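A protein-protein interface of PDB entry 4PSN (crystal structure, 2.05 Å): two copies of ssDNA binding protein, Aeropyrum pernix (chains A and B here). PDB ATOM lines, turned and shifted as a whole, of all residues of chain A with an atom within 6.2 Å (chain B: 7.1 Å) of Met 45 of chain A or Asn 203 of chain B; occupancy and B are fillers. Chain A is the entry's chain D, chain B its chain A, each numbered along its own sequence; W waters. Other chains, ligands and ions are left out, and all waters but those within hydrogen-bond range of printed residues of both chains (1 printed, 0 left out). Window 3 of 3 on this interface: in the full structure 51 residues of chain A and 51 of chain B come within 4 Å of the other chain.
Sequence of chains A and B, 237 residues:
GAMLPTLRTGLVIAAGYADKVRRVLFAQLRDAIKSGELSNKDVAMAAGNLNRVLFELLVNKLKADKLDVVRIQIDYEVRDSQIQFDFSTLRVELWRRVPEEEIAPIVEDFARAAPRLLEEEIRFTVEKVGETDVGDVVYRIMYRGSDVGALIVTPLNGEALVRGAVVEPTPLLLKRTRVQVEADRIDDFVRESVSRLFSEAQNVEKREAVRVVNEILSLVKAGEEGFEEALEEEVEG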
ATOM      1  N   ARG A  22      25.684  -7.383   5.928  1.00  0.00           N
ATOM      2  CA  ARG A  22      25.730  -7.347   7.382  1.00  0.00           C
ATOM      3  C   ARG A  22      27.102  -6.848   7.883  1.00  0.00           C
ATOM      4  O   ARG A  22      27.193  -5.971   8.745  1.00  0.00           O
ATOM      5  CB  ARG A  22      25.478  -8.749   7.934  1.00  0.00           C
ATOM      6  CG  ARG A  22      25.236  -8.782   9.448  1.00  0.00           C
ATOM      7  CD  ARG A  22      24.957 -10.228   9.934  1.00  0.00           C
ATOM      8  NE  ARG A  22      24.319 -10.255  11.260  1.00  0.00           N
ATOM      9  CZ  ARG A  22      24.986 -10.325  12.403  1.00  0.00           C
ATOM     10  NH1 ARG A  22      26.302 -10.383  12.389  1.00  0.00           N
ATOM     11  NH2 ARG A  22      24.337 -10.331  13.555  1.00  0.00           N
ATOM     12  N   ASN A  40      24.014  -3.522  19.170  1.00  0.00           N
ATOM     13  CA  ASN A  40      24.262  -4.578  18.197  1.00  0.00           C
ATOM     14  C   ASN A  40      22.947  -5.065  17.593  1.00  0.00           C
ATOM     15  O   ASN A  40      22.842  -5.245  16.381  1.00  0.00           O
ATOM     16  CB  ASN A  40      24.995  -5.748  18.852  1.00  0.00           C
ATOM     17  CG  ASN A  40      26.470  -5.466  19.073  1.00  0.00           C
ATOM     18  OD1 ASN A  40      27.159  -4.954  18.192  1.00  0.00           O
ATOM     19  ND2 ASN A  40      26.960  -5.796  20.257  1.00  0.00           N
ATOM     20  N   LYS A  41      21.950  -5.263  18.453  1.00  0.00           N
ATOM     21  CA  LYS A  41      20.634  -5.724  18.031  1.00  0.00           C
ATOM     22  C   LYS A  41      20.041  -4.794  16.985  1.00  0.00           C
ATOM     23  O   LYS A  41      19.476  -5.259  16.003  1.00  0.00           O
ATOM     24  CB  LYS A  41      19.678  -5.830  19.226  1.00  0.00           C
ATOM     25  CG  LYS A  41      18.283  -6.314  18.863  1.00  0.00           C
ATOM     26  CD  LYS A  41      17.305  -6.219  20.047  1.00  0.00           C
ATOM     27  CE  LYS A  41      16.464  -4.936  19.993  1.00  0.00           C
ATOM     28  NZ  LYS A  41      15.259  -4.980  20.890  1.00  0.00           N
ATOM     29  N   ASP A  42      20.166  -3.483  17.199  1.00  0.00           N
ATOM     30  CA  ASP A  42      19.633  -2.495  16.254  1.00  0.00           C
ATOM     31  C   ASP A  42      20.226  -2.719  14.872  1.00  0.00           C
ATOM     32  O   ASP A  42      19.524  -2.730  13.863  1.00  0.00           O
ATOM     33  CB  ASP A  42      19.982  -1.060  16.688  1.00  0.00           C
ATOM     34  CG  ASP A  42      19.176  -0.593  17.884  1.00  0.00           C
ATOM     35  OD1 ASP A  42      18.042  -1.098  18.049  1.00  0.00           O
ATOM     36  OD2 ASP A  42      19.674   0.280  18.644  1.00  0.00           O
ATOM     37  N   VAL A  43      21.535  -2.896  14.845  1.00  0.00           N
ATOM     38  CA  VAL A  43      22.267  -2.984  13.589  1.00  0.00           C
ATOM     39  C   VAL A  43      21.984  -4.322  12.899  1.00  0.00           C
ATOM     40  O   VAL A  43      21.840  -4.372  11.686  1.00  0.00           O
ATOM     41  CB  VAL A  43      23.784  -2.794  13.831  1.00  0.00           C
ATOM     42  CG1 VAL A  43      24.588  -3.014  12.549  1.00  0.00           C
ATOM     43  CG2 VAL A  43      24.045  -1.390  14.373  1.00  0.00           C
ATOM     44  N   ALA A  44      21.903  -5.397  13.679  1.00  0.00           N
ATOM     45  CA  ALA A  44      21.615  -6.721  13.133  1.00  0.00           C
ATOM     46  C   ALA A  44      20.230  -6.737  12.471  1.00  0.00           C
ATOM     47  O   ALA A  44      20.045  -7.329  11.402  1.00  0.00           O
ATOM     48  CB  ALA A  44      21.678  -7.779  14.244  1.00  0.00           C
ATOM     49  N   MET A  45      19.257  -6.109  13.128  1.00  0.00           N
ATOM     50  CA  MET A  45      17.897  -6.045  12.599  1.00  0.00           C
ATOM     51  C   MET A  45      17.829  -5.222  11.333  1.00  0.00           C
ATOM     52  O   MET A  45      17.117  -5.583  10.392  1.00  0.00           O
ATOM     53  CB  MET A  45      16.925  -5.469  13.627  1.00  0.00           C
ATOM     54  CG  MET A  45      16.851  -6.295  14.898  1.00  0.00           C
ATOM     55  SD  MET A  45      15.387  -5.673  16.041  1.00  0.00           S
ATOM     56  CE  MET A  45      13.954  -5.738  14.707  1.00  0.00           C
ATOM     57  N   ALA A  46      18.561  -4.107  11.310  1.00  0.00           N
ATOM     58  CA  ALA A  46      18.581  -3.266  10.118  1.00  0.00           C
ATOM     59  C   ALA A  46      19.179  -4.042   8.932  1.00  0.00           C
ATOM     60  O   ALA A  46      18.620  -4.064   7.837  1.00  0.00           O
ATOM     61  CB  ALA A  46      19.353  -1.971  10.385  1.00  0.00           C
ATOM     62  N   ALA A  47      20.310  -4.699   9.152  1.00  0.00           N
ATOM     63  CA  ALA A  47      20.902  -5.512   8.098  1.00  0.00           C
ATOM     64  C   ALA A  47      19.977  -6.669   7.683  1.00  0.00           C
ATOM     65  O   ALA A  47      19.845  -6.961   6.504  1.00  0.00           O
ATOM     66  CB  ALA A  47      22.274  -6.054   8.533  1.00  0.00           C
ATOM     67  N   GLY A  48      19.349  -7.321   8.662  1.00  0.00           N
ATOM     68  CA  GLY A  48      18.453  -8.427   8.376  1.00  0.00           C
ATOM     69  C   GLY A  48      17.235  -7.995   7.574  1.00  0.00           C
ATOM     70  O   GLY A  48      16.756  -8.728   6.698  1.00  0.00           O
ATOM     71  N   ASN A  49      16.719  -6.809   7.893  1.00  0.00           N
ATOM     72  CA  ASN A  49      15.590  -6.233   7.168  1.00  0.00           C
ATOM     73  C   ASN A  49      15.965  -5.932   5.723  1.00  0.00           C
ATOM     74  O   ASN A  49      15.210  -6.219   4.791  1.00  0.00           O
ATOM     75  CB  ASN A  49      15.122  -4.939   7.853  1.00  0.00           C
ATOM     76  CG  ASN A  49      14.289  -5.202   9.087  1.00  0.00           C
ATOM     77  OD1 ASN A  49      13.679  -6.263   9.228  1.00  0.00           O
ATOM     78  ND2 ASN A  49      14.251  -4.228   9.990  1.00  0.00           N
ATOM     79  N   LEU A  50      17.130  -5.325   5.545  1.00  0.00           N
ATOM     80  CA  LEU A  50      17.617  -5.029   4.201  1.00  0.00           C
ATOM     81  C   LEU A  50      17.855  -6.328   3.406  1.00  0.00           C
ATOM     82  O   LEU A  50      17.519  -6.406   2.227  1.00  0.00           O
ATOM     83  CB  LEU A  50      18.887  -4.166   4.246  1.00  0.00           C
ATOM     84  CG  LEU A  50      19.525  -3.890   2.887  1.00  0.00           C
ATOM     85  CD1 LEU A  50      18.574  -3.065   2.020  1.00  0.00           C
ATOM     86  CD2 LEU A  50      20.865  -3.168   3.055  1.00  0.00           C
ATOM     87  N   THR B 170      15.804 -14.199   4.993  1.00  0.00           N
ATOM     88  CA  THR B 170      16.917 -13.553   5.693  1.00  0.00           C
ATOM     89  C   THR B 170      17.395 -14.501   6.802  1.00  0.00           C
ATOM     90  O   THR B 170      16.585 -15.207   7.367  1.00  0.00           O
ATOM     91  CB  THR B 170      16.512 -12.178   6.279  1.00  0.00           C
ATOM     92  OG1 THR B 170      17.688 -11.467   6.675  1.00  0.00           O
ATOM     93  CG2 THR B 170      15.574 -12.349   7.503  1.00  0.00           C
ATOM     94  N   PRO B 171      18.716 -14.538   7.090  1.00  0.00           N
ATOM     95  CA  PRO B 171      19.207 -15.562   8.021  1.00  0.00           C
ATOM     96  C   PRO B 171      18.788 -15.288   9.462  1.00  0.00           C
ATOM     97  O   PRO B 171      19.047 -14.222  10.025  1.00  0.00           O
ATOM     98  CB  PRO B 171      20.735 -15.508   7.864  1.00  0.00           C
ATOM     99  CG  PRO B 171      20.974 -14.723   6.573  1.00  0.00           C
ATOM    100  CD  PRO B 171      19.817 -13.761   6.492  1.00  0.00           C
ATOM    101  N   LEU B 172      18.129 -16.276  10.053  1.00  0.00           N
ATOM    102  CA  LEU B 172      17.544 -16.122  11.375  1.00  0.00           C
ATOM    103  C   LEU B 172      17.942 -17.330  12.195  1.00  0.00           C
ATOM    104  O   LEU B 172      17.903 -18.459  11.697  1.00  0.00           O
ATOM    105  CB  LEU B 172      16.011 -16.094  11.276  1.00  0.00           C
ATOM    106  CG  LEU B 172      15.428 -14.905  10.514  1.00  0.00           C
ATOM    107  CD1 LEU B 172      13.895 -15.031  10.406  1.00  0.00           C
ATOM    108  CD2 LEU B 172      15.837 -13.613  11.209  1.00  0.00           C
ATOM    109  N   LEU B 173      18.324 -17.080  13.445  1.00  0.00           N
ATOM    110  CA  LEU B 173      18.644 -18.136  14.398  1.00  0.00           C
ATOM    111  C   LEU B 173      17.611 -18.092  15.531  1.00  0.00           C
ATOM    112  O   LEU B 173      17.460 -17.078  16.209  1.00  0.00           O
ATOM    113  CB  LEU B 173      20.071 -17.954  14.959  1.00  0.00           C
ATOM    114  CG  LEU B 173      20.385 -18.894  16.138  1.00  0.00           C
ATOM    115  CD1 LEU B 173      20.386 -20.339  15.667  1.00  0.00           C
ATOM    116  CD2 LEU B 173      21.721 -18.548  16.770  1.00  0.00           C
ATOM    117  N   SER B 199       9.371 -14.896  14.106  1.00  0.00           N
ATOM    118  CA  SER B 199       9.227 -13.439  14.126  1.00  0.00           C
ATOM    119  C   SER B 199      10.065 -12.827  15.252  1.00  0.00           C
ATOM    120  O   SER B 199      10.267 -11.622  15.291  1.00  0.00           O
ATOM    121  CB  SER B 199       7.771 -13.005  14.280  1.00  0.00           C
ATOM    122  OG  SER B 199       7.304 -13.280  15.591  1.00  0.00           O
ATOM    123  N   GLU B 200      10.563 -13.654  16.164  1.00  0.00           N
ATOM    124  CA  GLU B 200      11.389 -13.139  17.251  1.00  0.00           C
ATOM    125  C   GLU B 200      12.799 -13.738  17.260  1.00  0.00           C
ATOM    126  O   GLU B 200      13.545 -13.565  18.224  1.00  0.00           O
ATOM    127  CB  GLU B 200      10.693 -13.356  18.600  1.00  0.00           C
ATOM    128  CG  GLU B 200       9.429 -12.509  18.765  1.00  0.00           C
ATOM    129  CD  GLU B 200       8.759 -12.685  20.120  1.00  0.00           C
ATOM    130  OE1 GLU B 200       8.883 -13.781  20.714  1.00  0.00           O
ATOM    131  OE2 GLU B 200       8.113 -11.722  20.592  1.00  0.00           O
ATOM    132  N   ALA B 201      13.174 -14.409  16.173  1.00  0.00           N
ATOM    133  CA  ALA B 201      14.507 -15.001  16.084  1.00  0.00           C
ATOM    134  C   ALA B 201      15.571 -13.930  15.888  1.00  0.00           C
ATOM    135  O   ALA B 201      15.267 -12.782  15.606  1.00  0.00           O
ATOM    136  CB  ALA B 201      14.583 -15.999  14.955  1.00  0.00           C
ATOM    137  N   GLN B 202      16.827 -14.337  16.000  1.00  0.00           N
ATOM    138  CA  GLN B 202      17.947 -13.414  15.932  1.00  0.00           C
ATOM    139  C   GLN B 202      18.475 -13.322  14.501  1.00  0.00           C
ATOM    140  O   GLN B 202      18.630 -14.342  13.833  1.00  0.00           O
ATOM    141  CB  GLN B 202      19.041 -13.895  16.891  1.00  0.00           C
ATOM    142  CG  GLN B 202      20.267 -13.000  16.997  1.00  0.00           C
ATOM    143  CD  GLN B 202      21.304 -13.551  17.969  1.00  0.00           C
ATOM    144  OE1 GLN B 202      21.289 -14.737  18.303  1.00  0.00           O
ATOM    145  NE2 GLN B 202      22.208 -12.688  18.429  1.00  0.00           N
ATOM    146  N   ASN B 203      18.742 -12.100  14.039  1.00  0.00           N
ATOM    147  CA  ASN B 203      19.387 -11.883  12.744  1.00  0.00           C
ATOM    148  C   ASN B 203      20.864 -12.227  12.837  1.00  0.00           C
ATOM    149  O   ASN B 203      21.589 -11.658  13.643  1.00  0.00           O
ATOM    150  CB  ASN B 203      19.181 -10.432  12.274  1.00  0.00           C
ATOM    151  CG  ASN B 203      17.719 -10.101  12.046  1.00  0.00           C
ATOM    152  OD1 ASN B 203      17.143 -10.469  11.019  1.00  0.00           O
ATOM    153  ND2 ASN B 203      17.107  -9.423  13.003  1.00  0.00           N
ATOM    154  N   VAL B 204      21.304 -13.196  12.044  1.00  0.00           N
ATOM    155  CA  VAL B 204      22.678 -13.669  12.132  1.00  0.00           C
ATOM    156  C   VAL B 204      23.306 -13.714  10.743  1.00  0.00           C
ATOM    157  O   VAL B 204      22.685 -13.313   9.762  1.00  0.00           O
ATOM    158  CB  VAL B 204      22.753 -15.090  12.780  1.00  0.00           C
ATOM    159  CG1 VAL B 204      22.320 -15.021  14.218  1.00  0.00           C
ATOM    160  CG2 VAL B 204      21.884 -16.097  11.986  1.00  0.00           C
ATOM    161  N   GLU B 205      24.552 -14.175  10.661  1.00  0.00           N
ATOM    162  CA  GLU B 205      25.179 -14.385   9.360  1.00  0.00           C
ATOM    163  C   GLU B 205      24.592 -15.617   8.713  1.00  0.00           C
ATOM    164  O   GLU B 205      24.190 -16.565   9.395  1.00  0.00           O
ATOM    165  CB  GLU B 205      26.699 -14.540   9.496  1.00  0.00           C
ATOM    166  CG  GLU B 205      27.388 -13.265   9.921  1.00  0.00           C
ATOM    167  CD  GLU B 205      28.897 -13.307   9.741  1.00  0.00           C
ATOM    168  OE1 GLU B 205      29.448 -14.389   9.425  1.00  0.00           O
ATOM    169  OE2 GLU B 205      29.530 -12.244   9.921  1.00  0.00           O
ATOM    170  N   GLU B 208      26.215 -18.878   9.660  1.00  0.00           N
ATOM    171  CA  GLU B 208      25.813 -19.457  10.934  1.00  0.00           C
ATOM    172  C   GLU B 208      24.506 -20.227  10.769  1.00  0.00           C
ATOM    173  O   GLU B 208      24.372 -21.363  11.242  1.00  0.00           O
ATOM    174  CB  GLU B 208      25.641 -18.355  11.969  1.00  0.00           C
ATOM    175  CG  GLU B 208      26.880 -17.506  12.150  1.00  0.00           C
ATOM    176  CD  GLU B 208      26.699 -16.461  13.233  1.00  0.00           C
ATOM    177  OE1 GLU B 208      26.396 -15.292  12.890  1.00  0.00           O
ATOM    178  OE2 GLU B 208      26.847 -16.820  14.429  1.00  0.00           O
HETATM  179  O   HOH W   1      28.256  -9.905  10.464  1.00  0.00           O
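The backbone carbonyl oxygen (O) of Pro 171 of chain B is in hydrogen-bond range of the backbone NH (N) of Val 204 of chain B (3.2 Å). N of Glu 205 of chain B is in hydrogen-bond range of OE1 of Glu 208 of chain B (3.1 Å). The backbone carbonyl oxygen (O) of Met 45 of chain A lies close to the side-chain amide nitrogen (ND2) of Asn 49 of chain A.
Met 45 of chain A touches just one residue of chain B: Asn 203 (3.5 Å). Printed residues of chain A within 4 Å of Thr 170 of chain B: Gly 48 (2.9 Å). Of the printed residues of chain A, Val 204 of chain B touches Arg 22. Of the printed residues of chain A, Glu 205 of chain B touches Arg 22. Printed residues of chain B within 4 Å of Arg 22 of chain A: Asn 203, Val 204 and Glu 205. Of the printed residues of chain B, Ala 44 of chain A touches Asn 203 (3.3 Å). The nearest residue of chain A that does not touch Asn 203 of chain B is Asn 49 of chain A (4.8 Å). The nearest printed residue of chain A that does not touch Glu 205 of chain B is Ala 44 of chain A (7.9 Å).
NE of Arg 22 of chain A touches C of Val 204 of chain B, 3.6 Å away. Arg 22 of chain A touches Glu 205 of chain B (CD to CG, 3.9 Å). O of Ala 44 of chain A touches CB of Asn 203 of chain B, at 3.3 Å. CA of Met 45 of chain A touches ND2 of Asn 203 of chain B, 3.5 Å away. Asn 203 of chain B touches Gly 48 of chain A (OD1 to CA, 3.6 Å).
No position is printed for both chains.
Of the 12 printed residues of chain B, 4 touch a printed residue of chain A. Hydrophobic or aromatic side chains of chain A within 4 Å of the printed part of chain B: Ala 44 and Met 45. Along chain A the printed residues that touch a printed residue of chain B span positions 22 to 48. Among the printed residues, no Asp or Glu carboxylate lies within 4 Å of a Lys or Arg side-chain nitrogen of the other chain.
Water W1 bridges OE2 of Glu 205 of chain B and NH1 of Arg 22 of chain A.
O of Gly 48 of chain A lies within hydrogen-bond range of OG1 of Thr 170 of chain B, 2.9 Å away. O of Asn 203 of chain B is in hydrogen-bond range of NH2 of Arg 22 of chain A, at 3.1 Å.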
